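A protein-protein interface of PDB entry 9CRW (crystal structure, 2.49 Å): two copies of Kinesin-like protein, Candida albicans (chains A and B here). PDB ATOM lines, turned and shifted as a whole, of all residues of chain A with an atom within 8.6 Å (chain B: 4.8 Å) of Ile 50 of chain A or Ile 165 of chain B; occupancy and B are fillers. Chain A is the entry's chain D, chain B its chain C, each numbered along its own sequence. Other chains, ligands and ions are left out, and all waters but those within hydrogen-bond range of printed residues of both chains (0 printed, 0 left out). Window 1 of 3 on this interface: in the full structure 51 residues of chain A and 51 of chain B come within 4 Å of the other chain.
Position printed for both chains: 161.
Of the 5 pairs that touch across the chains among the printed residues, none has its exchanged pair printed and touching as well.
Ile 50 of chain A touches just these residues of chain B: Ile 165 and His 166.
Ile 165 of chain B touches one residue of chain A.
Of chain A, only Ile 50 (3.7 Å) comes within 4 Å of His 166 of chain B.
Of the printed residues of chain A, Phe 172 of chain B touches Leu 54.
Of the printed residues of chain A, Ser 169 of chain B touches Leu 54.
Of the printed residues of chain B, Leu 54 of chain A touches Ser 169 (3.9 Å) and Phe 172 (3.9 Å).
Of the printed residues of chain B, Lys 43 of chain A touches Asp 162 (3.2 Å).
Printed residues of chain A that touch a printed residue of chain B: Lys 43, Ile 50 and Leu 54.
Hydrophobic or aromatic side chains of chain A within 4 Å of the printed part of chain B: Ile 50 and Leu 54.
Of the 10 printed residues of chain B, 5 touch a printed residue of chain A.
Among the printed residues, 5 pairs touch across the chains.
Among the printed residues, Asp or Glu carboxylates within 4 Å of a Lys or Arg side-chain nitrogen of the other chain: Lys 43 of chain A with Asp 162 of chain B (3.2 Å).
Ile 165 of chain B touches Ile 50 of chain A.
CE1 of His 166 of chain B touches CG1 of Ile 50 of chain A (3.7 Å).
O of Ser 169 of chain B touches CD1 of Leu 54 of chain A, at 3.9 Å.
Phe 172 of chain B touches Leu 54 of chain A (CB to CD1, 3.9 Å).
The side-chain carboxylate (OD2) of Asp 162 of chain B lies within salt-bridge range of the side-chain amino group (NZ) of Lys 43 of chain A.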
ATOM      1  N   LYS A  43      23.140 -16.524   9.404  1.00  0.00           N
ATOM      2  CA  LYS A  43      22.146 -17.047  10.354  1.00  0.00           C
ATOM      3  C   LYS A  43      20.871 -16.193  10.369  1.00  0.00           C
ATOM      4  O   LYS A  43      19.740 -16.726  10.417  1.00  0.00           O
ATOM      5  CB  LYS A  43      22.738 -17.166  11.768  1.00  0.00           C
ATOM      6  CG  LYS A  43      23.844 -18.241  11.895  1.00  0.00           C
ATOM      7  CD  LYS A  43      23.418 -19.402  12.759  1.00  0.00           C
ATOM      8  CE  LYS A  43      24.429 -20.555  12.681  1.00  0.00           C
ATOM      9  NZ  LYS A  43      24.229 -21.564  13.758  1.00  0.00           N
ATOM     10  N   LEU A  44      21.035 -14.862  10.326  1.00  0.00           N
ATOM     11  CA  LEU A  44      19.872 -13.987  10.216  1.00  0.00           C
ATOM     12  C   LEU A  44      19.016 -14.334   8.984  1.00  0.00           C
ATOM     13  O   LEU A  44      17.772 -14.398   9.062  1.00  0.00           O
ATOM     14  CB  LEU A  44      20.337 -12.540  10.187  1.00  0.00           C
ATOM     15  CG  LEU A  44      20.703 -11.983  11.565  1.00  0.00           C
ATOM     16  CD1 LEU A  44      21.400 -10.628  11.443  1.00  0.00           C
ATOM     17  CD2 LEU A  44      19.448 -11.843  12.398  1.00  0.00           C
ATOM     18  N   LEU A  45      19.659 -14.615   7.850  1.00  0.00           N
ATOM     19  CA  LEU A  45      18.849 -14.806   6.651  1.00  0.00           C
ATOM     20  C   LEU A  45      18.191 -16.174   6.643  1.00  0.00           C
ATOM     21  O   LEU A  45      17.045 -16.302   6.171  1.00  0.00           O
ATOM     22  CB  LEU A  45      19.683 -14.578   5.382  1.00  0.00           C
ATOM     23  CG  LEU A  45      20.286 -13.178   5.265  1.00  0.00           C
ATOM     24  CD1 LEU A  45      21.206 -13.071   4.072  1.00  0.00           C
ATOM     25  CD2 LEU A  45      19.177 -12.151   5.188  1.00  0.00           C
ATOM     26  N   LEU A  46      18.893 -17.199   7.153  1.00  0.00           N
ATOM     27  CA  LEU A  46      18.282 -18.522   7.321  1.00  0.00           C
ATOM     28  C   LEU A  46      17.049 -18.462   8.232  1.00  0.00           C
ATOM     29  O   LEU A  46      16.002 -19.083   7.949  1.00  0.00           O
ATOM     30  CB  LEU A  46      19.335 -19.472   7.866  1.00  0.00           C
ATOM     31  CG  LEU A  46      20.043 -20.457   6.902  1.00  0.00           C
ATOM     32  CD1 LEU A  46      20.608 -19.842   5.645  1.00  0.00           C
ATOM     33  CD2 LEU A  46      21.170 -21.218   7.632  1.00  0.00           C
ATOM     34  N   SER A  47      17.113 -17.637   9.273  1.00  0.00           N
ATOM     35  CA  SER A  47      15.926 -17.471  10.096  1.00  0.00           C
ATOM     36  C   SER A  47      14.796 -16.797   9.305  1.00  0.00           C
ATOM     37  O   SER A  47      13.646 -17.287   9.289  1.00  0.00           O
ATOM     38  CB  SER A  47      16.292 -16.701  11.367  1.00  0.00           C
ATOM     39  OG  SER A  47      15.206 -16.703  12.283  1.00  0.00           O
ATOM     40  N   GLN A  48      15.111 -15.664   8.657  1.00  0.00           N
ATOM     41  CA  GLN A  48      14.115 -14.935   7.861  1.00  0.00           C
ATOM     42  C   GLN A  48      13.426 -15.863   6.860  1.00  0.00           C
ATOM     43  O   GLN A  48      12.191 -15.864   6.722  1.00  0.00           O
ATOM     44  CB  GLN A  48      14.794 -13.767   7.150  1.00  0.00           C
ATOM     45  CG  GLN A  48      13.910 -12.815   6.435  1.00  0.00           C
ATOM     46  CD  GLN A  48      14.679 -11.536   6.054  1.00  0.00           C
ATOM     47  OE1 GLN A  48      14.928 -11.253   4.865  1.00  0.00           O
ATOM     48  NE2 GLN A  48      15.078 -10.764   7.075  1.00  0.00           N
ATOM     49  N   LYS A  49      14.228 -16.687   6.178  1.00  0.00           N
ATOM     50  CA  LYS A  49      13.699 -17.650   5.221  1.00  0.00           C
ATOM     51  C   LYS A  49      12.696 -18.594   5.866  1.00  0.00           C
ATOM     52  O   LYS A  49      11.605 -18.799   5.319  1.00  0.00           O
ATOM     53  CB  LYS A  49      14.826 -18.458   4.581  1.00  0.00           C
ATOM     54  CG  LYS A  49      14.265 -19.551   3.661  1.00  0.00           C
ATOM     55  CD  LYS A  49      15.352 -20.218   2.792  1.00  0.00           C
ATOM     56  CE  LYS A  49      14.788 -21.436   2.053  1.00  0.00           C
ATOM     57  NZ  LYS A  49      15.846 -22.365   1.552  1.00  0.00           N
ATOM     58  N   ILE A  50      13.067 -19.229   6.998  1.00  0.00           N
ATOM     59  CA  ILE A  50      12.162 -20.207   7.607  1.00  0.00           C
ATOM     60  C   ILE A  50      10.857 -19.551   8.032  1.00  0.00           C
ATOM     61  O   ILE A  50       9.762 -20.107   7.833  1.00  0.00           O
ATOM     62  CB  ILE A  50      12.841 -20.894   8.799  1.00  0.00           C
ATOM     63  CG1 ILE A  50      13.789 -21.981   8.296  1.00  0.00           C
ATOM     64  CG2 ILE A  50      11.795 -21.461   9.759  1.00  0.00           C
ATOM     65  CD1 ILE A  50      14.830 -22.381   9.329  1.00  0.00           C
ATOM     66  N   GLU A  51      10.955 -18.369   8.647  1.00  0.00           N
ATOM     67  CA  GLU A  51       9.756 -17.681   9.115  1.00  0.00           C
ATOM     68  C   GLU A  51       8.834 -17.291   7.940  1.00  0.00           C
ATOM     69  O   GLU A  51       7.586 -17.429   8.019  1.00  0.00           O
ATOM     70  CB  GLU A  51      10.210 -16.497   9.964  1.00  0.00           C
ATOM     71  CG  GLU A  51       9.224 -15.359  10.134  1.00  0.00           C
ATOM     72  CD  GLU A  51       9.882 -14.170  10.832  1.00  0.00           C
ATOM     73  OE1 GLU A  51      10.129 -14.278  12.059  1.00  0.00           O
ATOM     74  OE2 GLU A  51      10.185 -13.150  10.150  1.00  0.00           O
ATOM     75  N   THR A  52       9.433 -16.890   6.811  1.00  0.00           N
ATOM     76  CA  THR A  52       8.620 -16.587   5.638  1.00  0.00           C
ATOM     77  C   THR A  52       8.026 -17.852   5.015  1.00  0.00           C
ATOM     78  O   THR A  52       6.843 -17.868   4.630  1.00  0.00           O
ATOM     79  CB  THR A  52       9.447 -15.809   4.631  1.00  0.00           C
ATOM     80  OG1 THR A  52      10.048 -14.683   5.295  1.00  0.00           O
ATOM     81  CG2 THR A  52       8.554 -15.317   3.501  1.00  0.00           C
ATOM     82  N   GLU A  53       8.834 -18.914   4.886  1.00  0.00           N
ATOM     83  CA  GLU A  53       8.306 -20.210   4.461  1.00  0.00           C
ATOM     84  C   GLU A  53       7.102 -20.606   5.292  1.00  0.00           C
ATOM     85  O   GLU A  53       6.093 -21.084   4.758  1.00  0.00           O
ATOM     86  CB  GLU A  53       9.380 -21.285   4.550  1.00  0.00           C
ATOM     87  CG  GLU A  53      10.267 -21.344   3.307  1.00  0.00           C
ATOM     88  CD  GLU A  53      11.568 -22.134   3.505  1.00  0.00           C
ATOM     89  OE1 GLU A  53      12.062 -22.210   4.646  1.00  0.00           O
ATOM     90  OE2 GLU A  53      12.102 -22.685   2.514  1.00  0.00           O
ATOM     91  N   LEU A  54       7.191 -20.410   6.614  1.00  0.00           N
ATOM     92  CA  LEU A  54       6.103 -20.820   7.499  1.00  0.00           C
ATOM     93  C   LEU A  54       4.844 -19.999   7.245  1.00  0.00           C
ATOM     94  O   LEU A  54       3.723 -20.531   7.309  1.00  0.00           O
ATOM     95  CB  LEU A  54       6.547 -20.710   8.952  1.00  0.00           C
ATOM     96  CG  LEU A  54       6.800 -22.059   9.586  1.00  0.00           C
ATOM     97  CD1 LEU A  54       7.503 -21.838  10.921  1.00  0.00           C
ATOM     98  CD2 LEU A  54       5.454 -22.746   9.772  1.00  0.00           C
ATOM     99  N   VAL A  55       5.002 -18.701   6.971  1.00  0.00           N
ATOM    100  CA  VAL A  55       3.848 -17.929   6.485  1.00  0.00           C
ATOM    101  C   VAL A  55       3.268 -18.576   5.218  1.00  0.00           C
ATOM    102  O   VAL A  55       2.094 -18.982   5.178  1.00  0.00           O
ATOM    103  CB  VAL A  55       4.231 -16.455   6.244  1.00  0.00           C
ATOM    104  CG1 VAL A  55       3.117 -15.719   5.501  1.00  0.00           C
ATOM    105  CG2 VAL A  55       4.507 -15.773   7.570  1.00  0.00           C
ATOM    106  N   LEU A  56       4.107 -18.721   4.184  1.00  0.00           N
ATOM    107  CA  LEU A  56       3.631 -19.148   2.867  1.00  0.00           C
ATOM    108  C   LEU A  56       2.949 -20.507   2.917  1.00  0.00           C
ATOM    109  O   LEU A  56       2.113 -20.828   2.060  1.00  0.00           O
ATOM    110  CB  LEU A  56       4.814 -19.210   1.904  1.00  0.00           C
ATOM    111  CG  LEU A  56       4.555 -18.949   0.423  1.00  0.00           C
ATOM    112  CD1 LEU A  56       3.556 -17.789   0.186  1.00  0.00           C
ATOM    113  CD2 LEU A  56       5.905 -18.641  -0.209  1.00  0.00           C
ATOM    114  N   GLU A  57       3.320 -21.319   3.902  1.00  0.00           N
ATOM    115  CA  GLU A  57       2.819 -22.672   4.024  1.00  0.00           C
ATOM    116  C   GLU A  57       1.360 -22.724   4.443  1.00  0.00           C
ATOM    117  O   GLU A  57       0.715 -23.767   4.267  1.00  0.00           O
ATOM    118  CB  GLU A  57       3.655 -23.393   5.049  1.00  0.00           C
ATOM    119  CG  GLU A  57       4.270 -24.665   4.620  1.00  0.00           C
ATOM    120  CD  GLU A  57       4.995 -25.265   5.813  1.00  0.00           C
ATOM    121  OE1 GLU A  57       4.366 -26.051   6.582  1.00  0.00           O
ATOM    122  OE2 GLU A  57       6.178 -24.872   6.013  1.00  0.00           O
ATOM    123  N   LEU A  88      10.847 -12.644  -1.349  1.00  0.00           N
ATOM    124  CA  LEU A  88      11.841 -12.698  -0.278  1.00  0.00           C
ATOM    125  C   LEU A  88      12.573 -14.035  -0.272  1.00  0.00           C
ATOM    126  O   LEU A  88      13.811 -14.080  -0.142  1.00  0.00           O
ATOM    127  CB  LEU A  88      11.169 -12.457   1.075  1.00  0.00           C
ATOM    128  CG  LEU A  88      12.102 -12.245   2.263  1.00  0.00           C
ATOM    129  CD1 LEU A  88      13.056 -11.080   1.963  1.00  0.00           C
ATOM    130  CD2 LEU A  88      11.271 -11.965   3.496  1.00  0.00           C
ATOM    131  N   ILE A  89      11.819 -15.144  -0.369  1.00  0.00           N
ATOM    132  CA  ILE A  89      12.470 -16.454  -0.407  1.00  0.00           C
ATOM    133  C   ILE A  89      13.475 -16.511  -1.554  1.00  0.00           C
ATOM    134  O   ILE A  89      14.590 -17.018  -1.391  1.00  0.00           O
ATOM    135  CB  ILE A  89      11.426 -17.584  -0.495  1.00  0.00           C
ATOM    136  CG1 ILE A  89      10.664 -17.705   0.840  1.00  0.00           C
ATOM    137  CG2 ILE A  89      12.115 -18.904  -0.823  1.00  0.00           C
ATOM    138  CD1 ILE A  89       9.502 -18.696   0.847  1.00  0.00           C
ATOM    139  N   ILE A  92      16.658 -14.354  -0.744  1.00  0.00           N
ATOM    140  CA  ILE A  92      17.540 -14.993   0.226  1.00  0.00           C
ATOM    141  C   ILE A  92      18.239 -16.188  -0.406  1.00  0.00           C
ATOM    142  O   ILE A  92      19.461 -16.384  -0.236  1.00  0.00           O
ATOM    143  CB  ILE A  92      16.752 -15.391   1.489  1.00  0.00           C
ATOM    144  CG1 ILE A  92      16.262 -14.136   2.219  1.00  0.00           C
ATOM    145  CG2 ILE A  92      17.611 -16.237   2.437  1.00  0.00           C
ATOM    146  CD1 ILE A  92      15.483 -14.447   3.447  1.00  0.00           C
ATOM    147  N   TYR A 161      25.501 -11.795  16.354  1.00  0.00           N
ATOM    148  CA  TYR A 161      24.121 -12.126  16.024  1.00  0.00           C
ATOM    149  C   TYR A 161      23.185 -11.795  17.182  1.00  0.00           C
ATOM    150  O   TYR A 161      22.099 -11.229  16.969  1.00  0.00           O
ATOM    151  CB  TYR A 161      24.029 -13.596  15.645  1.00  0.00           C
ATOM    152  CG  TYR A 161      22.631 -14.152  15.463  1.00  0.00           C
ATOM    153  CD1 TYR A 161      21.854 -14.551  16.570  1.00  0.00           C
ATOM    154  CD2 TYR A 161      22.111 -14.362  14.189  1.00  0.00           C
ATOM    155  CE1 TYR A 161      20.568 -15.100  16.402  1.00  0.00           C
ATOM    156  CE2 TYR A 161      20.826 -14.923  14.004  1.00  0.00           C
ATOM    157  CZ  TYR A 161      20.057 -15.283  15.115  1.00  0.00           C
ATOM    158  OH  TYR A 161      18.792 -15.825  14.938  1.00  0.00           O
ATOM    159  N   ILE A 174       6.297  -9.440  12.041  1.00  0.00           N
ATOM    160  CA  ILE A 174       5.205 -10.400  12.142  1.00  0.00           C
ATOM    161  C   ILE A 174       4.786 -10.655  13.604  1.00  0.00           C
ATOM    162  O   ILE A 174       3.567 -10.625  13.909  1.00  0.00           O
ATOM    163  CB  ILE A 174       5.608 -11.624  11.297  1.00  0.00           C
ATOM    164  CG1 ILE A 174       4.827 -12.893  11.539  1.00  0.00           C
ATOM    165  CG2 ILE A 174       7.138 -11.820  11.205  1.00  0.00           C
ATOM    166  CD1 ILE A 174       5.108 -13.732  10.267  1.00  0.00           C
ATOM    167  N   TYR B 161      21.803 -26.434  16.365  1.00  0.00           N
ATOM    168  CA  TYR B 161      20.753 -25.418  16.311  1.00  0.00           C
ATOM    169  C   TYR B 161      20.188 -25.283  14.898  1.00  0.00           C
ATOM    170  O   TYR B 161      18.961 -25.225  14.709  1.00  0.00           O
ATOM    171  CB  TYR B 161      21.292 -24.079  16.799  1.00  0.00           C
ATOM    172  CG  TYR B 161      20.383 -22.902  16.520  1.00  0.00           C
ATOM    173  CD1 TYR B 161      20.393 -22.233  15.271  1.00  0.00           C
ATOM    174  CD2 TYR B 161      19.544 -22.426  17.500  1.00  0.00           C
ATOM    175  CE1 TYR B 161      19.566 -21.147  15.031  1.00  0.00           C
ATOM    176  CE2 TYR B 161      18.729 -21.325  17.272  1.00  0.00           C
ATOM    177  CZ  TYR B 161      18.732 -20.698  16.044  1.00  0.00           C
ATOM    178  OH  TYR B 161      17.893 -19.618  15.883  1.00  0.00           O
ATOM    179  N   ASP B 162      21.073 -25.183  13.892  1.00  0.00           N
ATOM    180  CA  ASP B 162      20.583 -25.121  12.515  1.00  0.00           C
ATOM    181  C   ASP B 162      19.556 -26.222  12.251  1.00  0.00           C
ATOM    182  O   ASP B 162      18.537 -25.985  11.589  1.00  0.00           O
ATOM    183  CB  ASP B 162      21.745 -25.199  11.507  1.00  0.00           C
ATOM    184  CG  ASP B 162      22.544 -23.868  11.391  1.00  0.00           C
ATOM    185  OD1 ASP B 162      23.712 -23.911  10.901  1.00  0.00           O
ATOM    186  OD2 ASP B 162      22.021 -22.790  11.808  1.00  0.00           O
ATOM    187  N   ASN B 163      19.783 -27.426  12.805  1.00  0.00           N
ATOM    188  CA  ASN B 163      18.848 -28.530  12.557  1.00  0.00           C
ATOM    189  C   ASN B 163      17.607 -28.463  13.446  1.00  0.00           C
ATOM    190  O   ASN B 163      16.491 -28.782  12.993  1.00  0.00           O
ATOM    191  CB  ASN B 163      19.558 -29.873  12.742  1.00  0.00           C
ATOM    192  CG  ASN B 163      20.327 -30.313  11.495  1.00  0.00           C
ATOM    193  OD1 ASN B 163      21.560 -30.237  11.436  1.00  0.00           O
ATOM    194  ND2 ASN B 163      19.590 -30.778  10.486  1.00  0.00           N
ATOM    195  N   LEU B 164      17.779 -28.048  14.701  1.00  0.00           N
ATOM    196  CA  LEU B 164      16.664 -28.014  15.638  1.00  0.00           C
ATOM    197  C   LEU B 164      15.624 -26.981  15.220  1.00  0.00           C
ATOM    198  O   LEU B 164      14.418 -27.201  15.431  1.00  0.00           O
ATOM    199  CB  LEU B 164      17.178 -27.734  17.056  1.00  0.00           C
ATOM    200  CG  LEU B 164      17.796 -28.909  17.822  1.00  0.00           C
ATOM    201  CD1 LEU B 164      18.262 -28.501  19.214  1.00  0.00           C
ATOM    202  CD2 LEU B 164      16.794 -30.027  17.944  1.00  0.00           C
ATOM    203  N   ILE B 165      16.069 -25.870  14.614  1.00  0.00           N
ATOM    204  CA  ILE B 165      15.135 -24.827  14.198  1.00  0.00           C
ATOM    205  C   ILE B 165      14.134 -25.398  13.202  1.00  0.00           C
ATOM    206  O   ILE B 165      12.951 -25.029  13.218  1.00  0.00           O
ATOM    207  CB  ILE B 165      15.888 -23.603  13.637  1.00  0.00           C
ATOM    208  CG1 ILE B 165      15.005 -22.360  13.719  1.00  0.00           C
ATOM    209  CG2 ILE B 165      16.367 -23.828  12.180  1.00  0.00           C
ATOM    210  CD1 ILE B 165      15.665 -21.073  13.225  1.00  0.00           C
ATOM    211  N   HIS B 166      14.572 -26.348  12.361  1.00  0.00           N
ATOM    212  CA  HIS B 166      13.692 -26.999  11.393  1.00  0.00           C
ATOM    213  C   HIS B 166      12.819 -28.053  12.044  1.00  0.00           C
ATOM    214  O   HIS B 166      11.607 -28.090  11.806  1.00  0.00           O
ATOM    215  CB  HIS B 166      14.499 -27.628  10.260  1.00  0.00           C
ATOM    216  CG  HIS B 166      14.509 -26.800   9.018  1.00  0.00           C
ATOM    217  ND1 HIS B 166      13.352 -26.295   8.460  1.00  0.00           N
ATOM    218  CD2 HIS B 166      15.530 -26.352   8.246  1.00  0.00           C
ATOM    219  CE1 HIS B 166      13.658 -25.591   7.384  1.00  0.00           C
ATOM    220  NE2 HIS B 166      14.973 -25.608   7.230  1.00  0.00           N
ATOM    221  N   ASP B 167      13.425 -28.936  12.844  1.00  0.00           N
ATOM    222  CA  ASP B 167      12.624 -29.923  13.562  1.00  0.00           C
ATOM    223  C   ASP B 167      11.510 -29.264  14.356  1.00  0.00           C
ATOM    224  O   ASP B 167      10.372 -29.758  14.373  1.00  0.00           O
ATOM    225  CB  ASP B 167      13.488 -30.740  14.514  1.00  0.00           C
ATOM    226  CG  ASP B 167      14.201 -31.868  13.831  1.00  0.00           C
ATOM    227  OD1 ASP B 167      13.721 -32.295  12.756  1.00  0.00           O
ATOM    228  OD2 ASP B 167      15.228 -32.332  14.381  1.00  0.00           O
ATOM    229  N   LEU B 168      11.824 -28.158  15.038  1.00  0.00           N
ATOM    230  CA  LEU B 168      10.918 -27.529  15.987  1.00  0.00           C
ATOM    231  C   LEU B 168       9.897 -26.609  15.313  1.00  0.00           C
ATOM    232  O   LEU B 168       9.254 -25.803  16.009  1.00  0.00           O
ATOM    233  CB  LEU B 168      11.725 -26.783  17.058  1.00  0.00           C
ATOM    234  CG  LEU B 168      12.475 -27.686  18.080  1.00  0.00           C
ATOM    235  CD1 LEU B 168      13.292 -26.903  19.128  1.00  0.00           C
ATOM    236  CD2 LEU B 168      11.565 -28.706  18.802  1.00  0.00           C
ATOM    237  N   SER B 169       9.689 -26.766  13.993  1.00  0.00           N
ATOM    238  CA  SER B 169       8.961 -25.767  13.213  1.00  0.00           C
ATOM    239  C   SER B 169       7.530 -25.604  13.703  1.00  0.00           C
ATOM    240  O   SER B 169       7.004 -24.490  13.713  1.00  0.00           O
ATOM    241  CB  SER B 169       8.980 -26.140  11.732  1.00  0.00           C
ATOM    242  OG  SER B 169       7.739 -26.728  11.348  1.00  0.00           O
ATOM    243  N   PHE B 172       6.649 -22.841  16.296  1.00  0.00           N
ATOM    244  CA  PHE B 172       6.745 -21.445  15.884  1.00  0.00           C
ATOM    245  C   PHE B 172       5.335 -21.003  15.520  1.00  0.00           C
ATOM    246  O   PHE B 172       4.932 -20.957  14.358  1.00  0.00           O
ATOM    247  CB  PHE B 172       7.714 -21.290  14.729  1.00  0.00           C
ATOM    248  CG  PHE B 172       9.099 -21.779  15.016  1.00  0.00           C
ATOM    249  CD1 PHE B 172       9.523 -22.020  16.323  1.00  0.00           C
ATOM    250  CD2 PHE B 172       9.994 -21.988  13.973  1.00  0.00           C
ATOM    251  CE1 PHE B 172      10.817 -22.473  16.584  1.00  0.00           C
ATOM    252  CE2 PHE B 172      11.276 -22.437  14.209  1.00  0.00           C
ATOM    253  CZ  PHE B 172      11.697 -22.679  15.529  1.00  0.00           C
